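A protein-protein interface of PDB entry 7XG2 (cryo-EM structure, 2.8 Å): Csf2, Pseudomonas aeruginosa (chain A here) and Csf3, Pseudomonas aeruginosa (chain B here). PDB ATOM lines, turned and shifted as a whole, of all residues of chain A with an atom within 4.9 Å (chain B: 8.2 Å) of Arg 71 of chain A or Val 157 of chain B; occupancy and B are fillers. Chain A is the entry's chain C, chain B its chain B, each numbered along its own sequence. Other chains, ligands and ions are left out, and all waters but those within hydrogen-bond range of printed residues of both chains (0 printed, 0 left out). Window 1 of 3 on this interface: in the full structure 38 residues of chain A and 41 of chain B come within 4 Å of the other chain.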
ATOM      1  N   GLY A  67     -29.516  -0.072 -16.662  1.00  0.00           N
ATOM      2  CA  GLY A  67     -28.933   1.247 -16.512  1.00  0.00           C
ATOM      3  C   GLY A  67     -27.966   1.338 -15.352  1.00  0.00           C
ATOM      4  O   GLY A  67     -27.071   2.184 -15.354  1.00  0.00           O
ATOM      5  N   ASN A  68     -28.136   0.476 -14.347  1.00  0.00           N
ATOM      6  CA  ASN A  68     -27.166   0.382 -13.263  1.00  0.00           C
ATOM      7  C   ASN A  68     -25.824  -0.127 -13.773  1.00  0.00           C
ATOM      8  O   ASN A  68     -24.766   0.387 -13.385  1.00  0.00           O
ATOM      9  CB  ASN A  68     -27.707  -0.535 -12.172  1.00  0.00           C
ATOM     10  CG  ASN A  68     -27.232  -0.144 -10.796  1.00  0.00           C
ATOM     11  OD1 ASN A  68     -26.676   0.934 -10.601  1.00  0.00           O
ATOM     12  ND2 ASN A  68     -27.441  -1.025  -9.832  1.00  0.00           N
ATOM     13  N   THR A  69     -25.857  -1.122 -14.662  1.00  0.00           N
ATOM     14  CA  THR A  69     -24.635  -1.689 -15.221  1.00  0.00           C
ATOM     15  C   THR A  69     -23.903  -0.680 -16.097  1.00  0.00           C
ATOM     16  O   THR A  69     -22.686  -0.512 -15.975  1.00  0.00           O
ATOM     17  CB  THR A  69     -24.974  -2.948 -16.019  1.00  0.00           C
ATOM     18  OG1 THR A  69     -25.596  -3.904 -15.152  1.00  0.00           O
ATOM     19  CG2 THR A  69     -23.724  -3.560 -16.614  1.00  0.00           C
ATOM     20  N   MET A  70     -24.635   0.029 -16.958  1.00  0.00           N
ATOM     21  CA  MET A  70     -24.013   1.038 -17.808  1.00  0.00           C
ATOM     22  C   MET A  70     -23.576   2.256 -17.005  1.00  0.00           C
ATOM     23  O   MET A  70     -22.585   2.906 -17.359  1.00  0.00           O
ATOM     24  CB  MET A  70     -24.978   1.446 -18.917  1.00  0.00           C
ATOM     25  CG  MET A  70     -25.458   0.290 -19.782  1.00  0.00           C
ATOM     26  SD  MET A  70     -24.163  -0.479 -20.769  1.00  0.00           S
ATOM     27  CE  MET A  70     -23.503   0.920 -21.657  1.00  0.00           C
ATOM     28  N   ARG A  71     -24.288   2.565 -15.918  1.00  0.00           N
ATOM     29  CA  ARG A  71     -23.886   3.646 -15.024  1.00  0.00           C
ATOM     30  C   ARG A  71     -22.571   3.329 -14.331  1.00  0.00           C
ATOM     31  O   ARG A  71     -21.666   4.173 -14.277  1.00  0.00           O
ATOM     32  CB  ARG A  71     -24.991   3.896 -14.001  1.00  0.00           C
ATOM     33  CG  ARG A  71     -24.765   5.087 -13.107  1.00  0.00           C
ATOM     34  CD  ARG A  71     -25.922   5.269 -12.149  1.00  0.00           C
ATOM     35  NE  ARG A  71     -25.688   6.368 -11.221  1.00  0.00           N
ATOM     36  CZ  ARG A  71     -26.008   7.631 -11.462  1.00  0.00           C
ATOM     37  NH1 ARG A  71     -26.587   7.993 -12.594  1.00  0.00           N
ATOM     38  NH2 ARG A  71     -25.741   8.553 -10.543  1.00  0.00           N
ATOM     39  N   SER A  72     -22.434   2.101 -13.829  1.00  0.00           N
ATOM     40  CA  SER A  72     -21.175   1.706 -13.214  1.00  0.00           C
ATOM     41  C   SER A  72     -20.078   1.545 -14.256  1.00  0.00           C
ATOM     42  O   SER A  72     -18.903   1.744 -13.948  1.00  0.00           O
ATOM     43  CB  SER A  72     -21.355   0.421 -12.422  1.00  0.00           C
ATOM     44  OG  SER A  72     -20.285   0.228 -11.515  1.00  0.00           O
ATOM     45  N   LEU A  73     -20.441   1.205 -15.495  1.00  0.00           N
ATOM     46  CA  LEU A  73     -19.447   1.127 -16.561  1.00  0.00           C
ATOM     47  C   LEU A  73     -18.893   2.504 -16.903  1.00  0.00           C
ATOM     48  O   LEU A  73     -17.679   2.664 -17.072  1.00  0.00           O
ATOM     49  CB  LEU A  73     -20.056   0.466 -17.796  1.00  0.00           C
ATOM     50  CG  LEU A  73     -19.249   0.598 -19.088  1.00  0.00           C
ATOM     51  CD1 LEU A  73     -18.020  -0.292 -19.056  1.00  0.00           C
ATOM     52  CD2 LEU A  73     -20.097   0.291 -20.290  1.00  0.00           C
ATOM     53  N   LEU A  74     -19.770   3.512 -16.987  1.00  0.00           N
ATOM     54  CA  LEU A  74     -19.336   4.892 -17.196  1.00  0.00           C
ATOM     55  C   LEU A  74     -18.487   5.390 -16.033  1.00  0.00           C
ATOM     56  O   LEU A  74     -17.449   6.040 -16.241  1.00  0.00           O
ATOM     57  CB  LEU A  74     -20.555   5.796 -17.377  1.00  0.00           C
ATOM     58  CG  LEU A  74     -20.346   7.197 -17.949  1.00  0.00           C
ATOM     59  CD1 LEU A  74     -20.027   7.141 -19.414  1.00  0.00           C
ATOM     60  CD2 LEU A  74     -21.570   8.035 -17.728  1.00  0.00           C
ATOM     61  N   ARG A  75     -18.909   5.068 -14.801  1.00  0.00           N
ATOM     62  CA  ARG A  75     -18.154   5.435 -13.608  1.00  0.00           C
ATOM     63  C   ARG A  75     -16.768   4.808 -13.612  1.00  0.00           C
ATOM     64  O   ARG A  75     -15.763   5.505 -13.425  1.00  0.00           O
ATOM     65  CB  ARG A  75     -18.928   5.001 -12.363  1.00  0.00           C
ATOM     66  CG  ARG A  75     -18.245   5.302 -11.053  1.00  0.00           C
ATOM     67  CD  ARG A  75     -18.720   4.356  -9.972  1.00  0.00           C
ATOM     68  NE  ARG A  75     -20.143   4.502  -9.691  1.00  0.00           N
ATOM     69  CZ  ARG A  75     -20.649   5.372  -8.829  1.00  0.00           C
ATOM     70  NH1 ARG A  75     -19.875   6.202  -8.151  1.00  0.00           N
ATOM     71  NH2 ARG A  75     -21.964   5.412  -8.642  1.00  0.00           N
ATOM     72  N   LEU A 132     -21.553  13.967 -10.676  1.00  0.00           N
ATOM     73  CA  LEU A 132     -22.203  13.076 -11.633  1.00  0.00           C
ATOM     74  C   LEU A 132     -22.950  11.949 -10.931  1.00  0.00           C
ATOM     75  O   LEU A 132     -24.067  11.597 -11.319  1.00  0.00           O
ATOM     76  CB  LEU A 132     -21.174  12.508 -12.607  1.00  0.00           C
ATOM     77  CG  LEU A 132     -20.607  13.486 -13.632  1.00  0.00           C
ATOM     78  CD1 LEU A 132     -19.598  12.785 -14.520  1.00  0.00           C
ATOM     79  CD2 LEU A 132     -21.725  14.087 -14.453  1.00  0.00           C
ATOM     80  N   PHE A 133     -22.361  11.372  -9.890  1.00  0.00           N
ATOM     81  CA  PHE A 133     -23.001  10.246  -9.224  1.00  0.00           C
ATOM     82  C   PHE A 133     -23.439  10.556  -7.810  1.00  0.00           C
ATOM     83  O   PHE A 133     -24.496  10.080  -7.386  1.00  0.00           O
ATOM     84  CB  PHE A 133     -22.062   9.041  -9.203  1.00  0.00           C
ATOM     85  CG  PHE A 133     -21.642   8.605 -10.559  1.00  0.00           C
ATOM     86  CD1 PHE A 133     -22.472   7.813 -11.334  1.00  0.00           C
ATOM     87  CD2 PHE A 133     -20.433   9.017 -11.077  1.00  0.00           C
ATOM     88  CE1 PHE A 133     -22.087   7.428 -12.595  1.00  0.00           C
ATOM     89  CE2 PHE A 133     -20.053   8.638 -12.325  1.00  0.00           C
ATOM     90  CZ  PHE A 133     -20.878   7.850 -13.095  1.00  0.00           C
ATOM     91  N   GLY A 142     -26.991  12.694  -8.092  1.00  0.00           N
ATOM     92  CA  GLY A 142     -26.103  12.988  -9.186  1.00  0.00           C
ATOM     93  C   GLY A 142     -26.732  13.873 -10.241  1.00  0.00           C
ATOM     94  O   GLY A 142     -27.949  13.937 -10.394  1.00  0.00           O
ATOM     95  N   LEU A 144     -26.223  13.150 -13.238  1.00  0.00           N
ATOM     96  CA  LEU A 144     -26.171  12.256 -14.382  1.00  0.00           C
ATOM     97  C   LEU A 144     -27.241  11.178 -14.289  1.00  0.00           C
ATOM     98  O   LEU A 144     -27.393  10.530 -13.251  1.00  0.00           O
ATOM     99  CB  LEU A 144     -24.788  11.617 -14.445  1.00  0.00           C
ATOM    100  CG  LEU A 144     -24.286  10.774 -15.595  1.00  0.00           C
ATOM    101  CD1 LEU A 144     -23.629  11.665 -16.598  1.00  0.00           C
ATOM    102  CD2 LEU A 144     -23.287   9.832 -15.007  1.00  0.00           C
ATOM    103  N   MET A 145     -27.980  10.997 -15.377  1.00  0.00           N
ATOM    104  CA  MET A 145     -28.808   9.823 -15.598  1.00  0.00           C
ATOM    105  C   MET A 145     -28.136   8.989 -16.671  1.00  0.00           C
ATOM    106  O   MET A 145     -27.798   9.508 -17.740  1.00  0.00           O
ATOM    107  CB  MET A 145     -30.222  10.190 -16.045  1.00  0.00           C
ATOM    108  CG  MET A 145     -31.025   8.972 -16.484  1.00  0.00           C
ATOM    109  SD  MET A 145     -31.964   9.040 -18.030  1.00  0.00           S
ATOM    110  CE  MET A 145     -30.703   9.302 -19.263  1.00  0.00           C
ATOM    111  N   VAL A 146     -27.931   7.713 -16.383  1.00  0.00           N
ATOM    112  CA  VAL A 146     -27.446   6.755 -17.360  1.00  0.00           C
ATOM    113  C   VAL A 146     -28.552   5.743 -17.597  1.00  0.00           C
ATOM    114  O   VAL A 146     -28.845   4.918 -16.725  1.00  0.00           O
ATOM    115  CB  VAL A 146     -26.157   6.071 -16.887  1.00  0.00           C
ATOM    116  CG1 VAL A 146     -25.789   4.991 -17.839  1.00  0.00           C
ATOM    117  CG2 VAL A 146     -25.042   7.077 -16.784  1.00  0.00           C
ATOM    118  N   ASP A 147     -29.173   5.813 -18.765  1.00  0.00           N
ATOM    119  CA  ASP A 147     -30.259   4.906 -19.084  1.00  0.00           C
ATOM    120  C   ASP A 147     -29.709   3.533 -19.457  1.00  0.00           C
ATOM    121  O   ASP A 147     -28.503   3.333 -19.609  1.00  0.00           O
ATOM    122  CB  ASP A 147     -31.122   5.471 -20.213  1.00  0.00           C
ATOM    123  CG  ASP A 147     -32.564   5.006 -20.135  1.00  0.00           C
ATOM    124  OD1 ASP A 147     -32.847   4.072 -19.354  1.00  0.00           O
ATOM    125  OD2 ASP A 147     -33.413   5.567 -20.854  1.00  0.00           O
ATOM    126  N   SER A 148     -30.625   2.577 -19.582  1.00  0.00           N
ATOM    127  CA  SER A 148     -30.303   1.229 -20.016  1.00  0.00           C
ATOM    128  C   SER A 148     -29.797   1.228 -21.450  1.00  0.00           C
ATOM    129  O   SER A 148     -30.095   2.143 -22.222  1.00  0.00           O
ATOM    130  CB  SER A 148     -31.533   0.333 -19.893  1.00  0.00           C
ATOM    131  OG  SER A 148     -31.970   0.243 -18.549  1.00  0.00           O
ATOM    132  N   ASN B  12     -40.167   4.291 -20.859  1.00  0.00           N
ATOM    133  CA  ASN B  12     -39.488   3.343 -19.995  1.00  0.00           C
ATOM    134  C   ASN B  12     -40.424   2.925 -18.867  1.00  0.00           C
ATOM    135  O   ASN B  12     -41.249   3.720 -18.420  1.00  0.00           O
ATOM    136  CB  ASN B  12     -38.232   3.969 -19.398  1.00  0.00           C
ATOM    137  CG  ASN B  12     -37.075   4.023 -20.374  1.00  0.00           C
ATOM    138  OD1 ASN B  12     -36.019   3.454 -20.120  1.00  0.00           O
ATOM    139  ND2 ASN B  12     -37.258   4.729 -21.484  1.00  0.00           N
ATOM    140  N   PRO B  13     -40.321   1.690 -18.388  1.00  0.00           N
ATOM    141  CA  PRO B  13     -41.011   1.333 -17.145  1.00  0.00           C
ATOM    142  C   PRO B  13     -40.356   2.022 -15.958  1.00  0.00           C
ATOM    143  O   PRO B  13     -39.219   2.488 -16.029  1.00  0.00           O
ATOM    144  CB  PRO B  13     -40.850  -0.189 -17.067  1.00  0.00           C
ATOM    145  CG  PRO B  13     -40.454  -0.615 -18.444  1.00  0.00           C
ATOM    146  CD  PRO B  13     -39.678   0.525 -19.011  1.00  0.00           C
ATOM    147  N   MET B  15     -39.927   2.182 -11.415  1.00  0.00           N
ATOM    148  CA  MET B  15     -40.030   1.438 -10.169  1.00  0.00           C
ATOM    149  C   MET B  15     -41.458   1.529  -9.665  1.00  0.00           C
ATOM    150  O   MET B  15     -42.051   2.611  -9.669  1.00  0.00           O
ATOM    151  CB  MET B  15     -39.080   2.005  -9.118  1.00  0.00           C
ATOM    152  CG  MET B  15     -37.752   2.482  -9.637  1.00  0.00           C
ATOM    153  SD  MET B  15     -36.838   1.433 -10.770  1.00  0.00           S
ATOM    154  CE  MET B  15     -36.225   0.180  -9.663  1.00  0.00           C
ATOM    155  N   TRP B  82     -37.014  -5.831 -10.879  1.00  0.00           N
ATOM    156  CA  TRP B  82     -35.668  -5.442 -11.261  1.00  0.00           C
ATOM    157  C   TRP B  82     -34.705  -5.868 -10.170  1.00  0.00           C
ATOM    158  O   TRP B  82     -34.721  -5.309  -9.068  1.00  0.00           O
ATOM    159  CB  TRP B  82     -35.563  -3.937 -11.488  1.00  0.00           C
ATOM    160  CG  TRP B  82     -34.527  -3.539 -12.482  1.00  0.00           C
ATOM    161  CD1 TRP B  82     -33.457  -2.728 -12.258  1.00  0.00           C
ATOM    162  CD2 TRP B  82     -34.457  -3.923 -13.860  1.00  0.00           C
ATOM    163  NE1 TRP B  82     -32.718  -2.588 -13.405  1.00  0.00           N
ATOM    164  CE2 TRP B  82     -33.312  -3.312 -14.404  1.00  0.00           C
ATOM    165  CE3 TRP B  82     -35.249  -4.726 -14.690  1.00  0.00           C
ATOM    166  CZ2 TRP B  82     -32.944  -3.476 -15.729  1.00  0.00           C
ATOM    167  CZ3 TRP B  82     -34.877  -4.890 -15.999  1.00  0.00           C
ATOM    168  CH2 TRP B  82     -33.735  -4.271 -16.506  1.00  0.00           C
ATOM    169  N   GLN B  84     -31.015  -5.568  -8.965  1.00  0.00           N
ATOM    170  CA  GLN B  84     -29.821  -4.762  -9.129  1.00  0.00           C
ATOM    171  C   GLN B  84     -28.853  -5.156  -8.033  1.00  0.00           C
ATOM    172  O   GLN B  84     -29.257  -5.700  -7.000  1.00  0.00           O
ATOM    173  CB  GLN B  84     -30.128  -3.266  -9.085  1.00  0.00           C
ATOM    174  CG  GLN B  84     -30.377  -2.634 -10.438  1.00  0.00           C
ATOM    175  CD  GLN B  84     -30.941  -1.234 -10.334  1.00  0.00           C
ATOM    176  OE1 GLN B  84     -30.946  -0.483 -11.306  1.00  0.00           O
ATOM    177  NE2 GLN B  84     -31.423  -0.877  -9.153  1.00  0.00           N
ATOM    178  N   TYR B 121     -30.545  -6.533  -4.504  1.00  0.00           N
ATOM    179  CA  TYR B 121     -31.796  -5.918  -4.089  1.00  0.00           C
ATOM    180  C   TYR B 121     -32.750  -5.878  -5.268  1.00  0.00           C
ATOM    181  O   TYR B 121     -32.354  -5.578  -6.397  1.00  0.00           O
ATOM    182  CB  TYR B 121     -31.594  -4.506  -3.513  1.00  0.00           C
ATOM    183  CG  TYR B 121     -30.975  -3.482  -4.441  1.00  0.00           C
ATOM    184  CD1 TYR B 121     -29.609  -3.481  -4.699  1.00  0.00           C
ATOM    185  CD2 TYR B 121     -31.752  -2.493  -5.028  1.00  0.00           C
ATOM    186  CE1 TYR B 121     -29.044  -2.553  -5.537  1.00  0.00           C
ATOM    187  CE2 TYR B 121     -31.191  -1.551  -5.862  1.00  0.00           C
ATOM    188  CZ  TYR B 121     -29.835  -1.581  -6.104  1.00  0.00           C
ATOM    189  OH  TYR B 121     -29.271  -0.649  -6.939  1.00  0.00           O
ATOM    190  N   GLN B 150     -38.474  12.364 -16.106  1.00  0.00           N
ATOM    191  CA  GLN B 150     -38.725  11.032 -15.573  1.00  0.00           C
ATOM    192  C   GLN B 150     -39.668  11.127 -14.386  1.00  0.00           C
ATOM    193  O   GLN B 150     -39.750  12.154 -13.712  1.00  0.00           O
ATOM    194  CB  GLN B 150     -37.447  10.326 -15.107  1.00  0.00           C
ATOM    195  CG  GLN B 150     -36.208  10.649 -15.892  1.00  0.00           C
ATOM    196  CD  GLN B 150     -35.067   9.750 -15.549  1.00  0.00           C
ATOM    197  OE1 GLN B 150     -33.918  10.124 -15.707  1.00  0.00           O
ATOM    198  NE2 GLN B 150     -35.375   8.534 -15.121  1.00  0.00           N
ATOM    199  N   GLY B 153     -39.196   6.398  -8.870  1.00  0.00           N
ATOM    200  CA  GLY B 153     -37.899   6.302  -8.238  1.00  0.00           C
ATOM    201  C   GLY B 153     -36.813   5.851  -9.194  1.00  0.00           C
ATOM    202  O   GLY B 153     -37.097   5.567 -10.358  1.00  0.00           O
ATOM    203  N   LYS B 154     -35.587   5.803  -8.657  1.00  0.00           N
ATOM    204  CA  LYS B 154     -34.367   5.342  -9.335  1.00  0.00           C
ATOM    205  C   LYS B 154     -34.191   5.988 -10.705  1.00  0.00           C
ATOM    206  O   LYS B 154     -34.039   5.317 -11.727  1.00  0.00           O
ATOM    207  CB  LYS B 154     -34.334   3.818  -9.429  1.00  0.00           C
ATOM    208  CG  LYS B 154     -34.453   3.133  -8.075  1.00  0.00           C
ATOM    209  CD  LYS B 154     -33.094   2.727  -7.530  1.00  0.00           C
ATOM    210  CE  LYS B 154     -33.179   2.359  -6.057  1.00  0.00           C
ATOM    211  NZ  LYS B 154     -34.461   1.682  -5.720  1.00  0.00           N
ATOM    212  N   ARG B 155     -34.240   7.316 -10.722  1.00  0.00           N
ATOM    213  CA  ARG B 155     -34.150   8.033 -11.984  1.00  0.00           C
ATOM    214  C   ARG B 155     -32.716   8.192 -12.458  1.00  0.00           C
ATOM    215  O   ARG B 155     -32.500   8.622 -13.593  1.00  0.00           O
ATOM    216  CB  ARG B 155     -34.821   9.395 -11.853  1.00  0.00           C
ATOM    217  CG  ARG B 155     -36.225   9.305 -11.304  1.00  0.00           C
ATOM    218  CD  ARG B 155     -36.721  10.651 -10.854  1.00  0.00           C
ATOM    219  NE  ARG B 155     -35.687  11.425 -10.181  1.00  0.00           N
ATOM    220  CZ  ARG B 155     -35.638  11.630  -8.873  1.00  0.00           C
ATOM    221  NH1 ARG B 155     -36.551  11.127  -8.060  1.00  0.00           N
ATOM    222  NH2 ARG B 155     -34.649  12.363  -8.368  1.00  0.00           N
ATOM    223  N   GLY B 156     -31.734   7.866 -11.618  1.00  0.00           N
ATOM    224  CA  GLY B 156     -30.351   7.916 -12.052  1.00  0.00           C
ATOM    225  C   GLY B 156     -29.966   6.794 -12.989  1.00  0.00           C
ATOM    226  O   GLY B 156     -29.001   6.939 -13.748  1.00  0.00           O
ATOM    227  N   VAL B 157     -30.693   5.683 -12.958  1.00  0.00           N
ATOM    228  CA  VAL B 157     -30.418   4.556 -13.835  1.00  0.00           C
ATOM    229  C   VAL B 157     -31.370   4.534 -15.033  1.00  0.00           C
ATOM    230  O   VAL B 157     -31.502   3.511 -15.701  1.00  0.00           O
ATOM    231  CB  VAL B 157     -30.446   3.225 -13.070  1.00  0.00           C
ATOM    232  CG1 VAL B 157     -29.333   3.197 -12.045  1.00  0.00           C
ATOM    233  CG2 VAL B 157     -31.779   3.015 -12.403  1.00  0.00           C
ATOM    234  N   GLY B 158     -32.014   5.660 -15.329  1.00  0.00           N
ATOM    235  CA  GLY B 158     -32.830   5.792 -16.515  1.00  0.00           C
ATOM    236  C   GLY B 158     -34.235   5.253 -16.414  1.00  0.00           C
ATOM    237  O   GLY B 158     -34.888   5.083 -17.449  1.00  0.00           O
ATOM    238  N   PHE B 159     -34.727   4.981 -15.214  1.00  0.00           N
ATOM    239  CA  PHE B 159     -36.011   4.321 -15.092  1.00  0.00           C
ATOM    240  C   PHE B 159     -37.143   5.339 -15.095  1.00  0.00           C
ATOM    241  O   PHE B 159     -37.008   6.455 -14.587  1.00  0.00           O
ATOM    242  CB  PHE B 159     -36.064   3.480 -13.820  1.00  0.00           C
ATOM    243  CG  PHE B 159     -35.878   2.018 -14.067  1.00  0.00           C
ATOM    244  CD1 PHE B 159     -34.609   1.466 -14.070  1.00  0.00           C
ATOM    245  CD2 PHE B 159     -36.963   1.191 -14.288  1.00  0.00           C
ATOM    246  CE1 PHE B 159     -34.428   0.123 -14.296  1.00  0.00           C
ATOM    247  CE2 PHE B 159     -36.788  -0.152 -14.526  1.00  0.00           C
ATOM    248  CZ  PHE B 159     -35.522  -0.687 -14.522  1.00  0.00           C
ATOM    249  N   GLY B 160     -38.267   4.940 -15.677  1.00  0.00           N
ATOM    250  CA  GLY B 160     -39.466   5.758 -15.684  1.00  0.00           C
ATOM    251  C   GLY B 160     -39.422   7.023 -16.509  1.00  0.00           C
ATOM    252  O   GLY B 160     -39.968   8.046 -16.083  1.00  0.00           O
ATOM    253  N   GLN B 161     -38.804   6.975 -17.688  1.00  0.00           N
ATOM    254  CA  GLN B 161     -38.708   8.148 -18.550  1.00  0.00           C
ATOM    255  C   GLN B 161     -40.079   8.500 -19.110  1.00  0.00           C
ATOM    256  O   GLN B 161     -40.739   7.657 -19.725  1.00  0.00           O
ATOM    257  CB  GLN B 161     -37.721   7.890 -19.682  1.00  0.00           C
ATOM    258  CG  GLN B 161     -36.274   7.887 -19.251  1.00  0.00           C
ATOM    259  CD  GLN B 161     -35.327   8.034 -20.419  1.00  0.00           C
ATOM    260  OE1 GLN B 161     -35.753   8.226 -21.557  1.00  0.00           O
ATOM    261  NE2 GLN B 161     -34.033   7.945 -20.146  1.00  0.00           N
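The side-chain amide nitrogen (NE2) of Gln 161 of chain B is in hydrogen-bond range of the side-chain carboxylate (OD2) of Asp 147 of chain A (2.6 Å).
The side-chain amide nitrogen (NE2) of Gln 161 of chain B lies within hydrogen-bond range of the side-chain sulfur (SD) of Met 145 of chain A (3.2 Å).
ND2 of Asn 68 of chain A is in hydrogen-bond range of OH of Tyr 121 of chain B, 3.4 Å away.
The backbone carbonyl oxygen of Gly 156 of chain B lies within hydrogen-bond range of the backbone NH of Val 146 of chain A, at 2.9 Å.
OD1 of Asp 147 of chain A lies close to O of Gly 158 of chain B, at 3.0 Å.
OE1 of Gln 150 of chain B sits close to SD of Met 145 of chain A.
The backbone carbonyl oxygen of Gly 156 of chain B lies within hydrogen-bond range of the guanidinium group of Arg 71 of chain A, 2.9 Å away.
The backbone carbonyl oxygen (O) of Val 146 of chain A lies close to the backbone carbonyl oxygen (O) of Val 157 of chain B (3.2 Å).
The side-chain amide oxygen of Asn 12 of chain B lies close to the side-chain carboxylate of Asp 147 of chain A, at 3.3 Å.
The indole nitrogen (NE1) of Trp 82 of chain B lies within hydrogen-bond range of the side-chain amide oxygen (OE1) of Gln 84 of chain B, 3.5 Å away.
OG of Ser 148 of chain A is in hydrogen-bond range of N of Gly 67 of chain A, at 3.1 Å.
OD1 of Asn 12 of chain B lies close to O of Gly 158 of chain B, 3.3 Å away.
NH1 of Arg 71 of chain A lies within hydrogen-bond range of O of Leu 144 of chain A, at 2.7 Å.
The backbone carbonyl oxygen (O) of Leu 132 of chain A lies close to the backbone NH (N) of Leu 144 of chain A, at 3.3 Å.
The backbone NH (N) of Gln 84 of chain B sits at hydrogen-bond distance from the backbone carbonyl oxygen (O) of Tyr 121 of chain B (2.9 Å).
Among the printed residues, pairs that only touch across the chains: Gly 67 of chain A with Val 157 of chain B (3.5 Å), Asn 68 of chain A with Gln 84 of chain B (3.4 Å), Asn 68 of chain A with Val 157 of chain B (3.8 Å), Arg 71 of chain A with Val 157 of chain B (3.99 Å), Leu 144 of chain A with Gly 156 of chain B (3.97 Å), Met 145 of chain A with Arg 155 of chain B (3.3 Å), Met 145 of chain A with Gly 156 of chain B (3.4 Å), Met 145 of chain A with Gly 158 of chain B (3.6 Å), Val 146 of chain A with Gly 158 of chain B (3.5 Å) and Asp 147 of chain A with Val 157 of chain B (3.9 Å).
Printed residues of chain B within 4 Å of Arg 71 of chain A: Gly 156 (2.9 Å) and Val 157 (3.99 Å).
Printed residues of chain A within 4 Å of Val 157 of chain B: Gly 67 (3.5 Å), Asn 68 (3.8 Å), Arg 71 (3.99 Å), Val 146 (3.1 Å) and Asp 147 (3.9 Å).
Printed residues of chain B within 4 Å of Met 145 of chain A: Gln 150, Arg 155, Gly 156, Gly 158 and Gln 161.
Printed residues of chain A within 4 Å of Asn 12 of chain B: Asp 147.
Of the printed residues of chain A, Gln 84 of chain B touches Asn 68.
Printed residues of chain A within 4 Å of Gln 161 of chain B: Met 145 (3.2 Å) and Asp 147 (2.6 Å).
Printed residues of chain B within 4 Å of Asp 147 of chain A: Asn 12, Val 157, Gly 158 and Gln 161.
Leu 132 of chain A touches none of the printed residues of chain B.
Met 70 of chain A touches none of the printed residues of chain B.
The nearest printed residue of chain A that does not touch Val 157 of chain B is Ser 148 of chain A (4.1 Å).
The nearest printed residue of chain A that does not touch Gln 150 of chain B is Val 146 of chain A (6.5 Å).
Of the 16 printed residues of chain B, 9 touch a printed residue of chain A.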
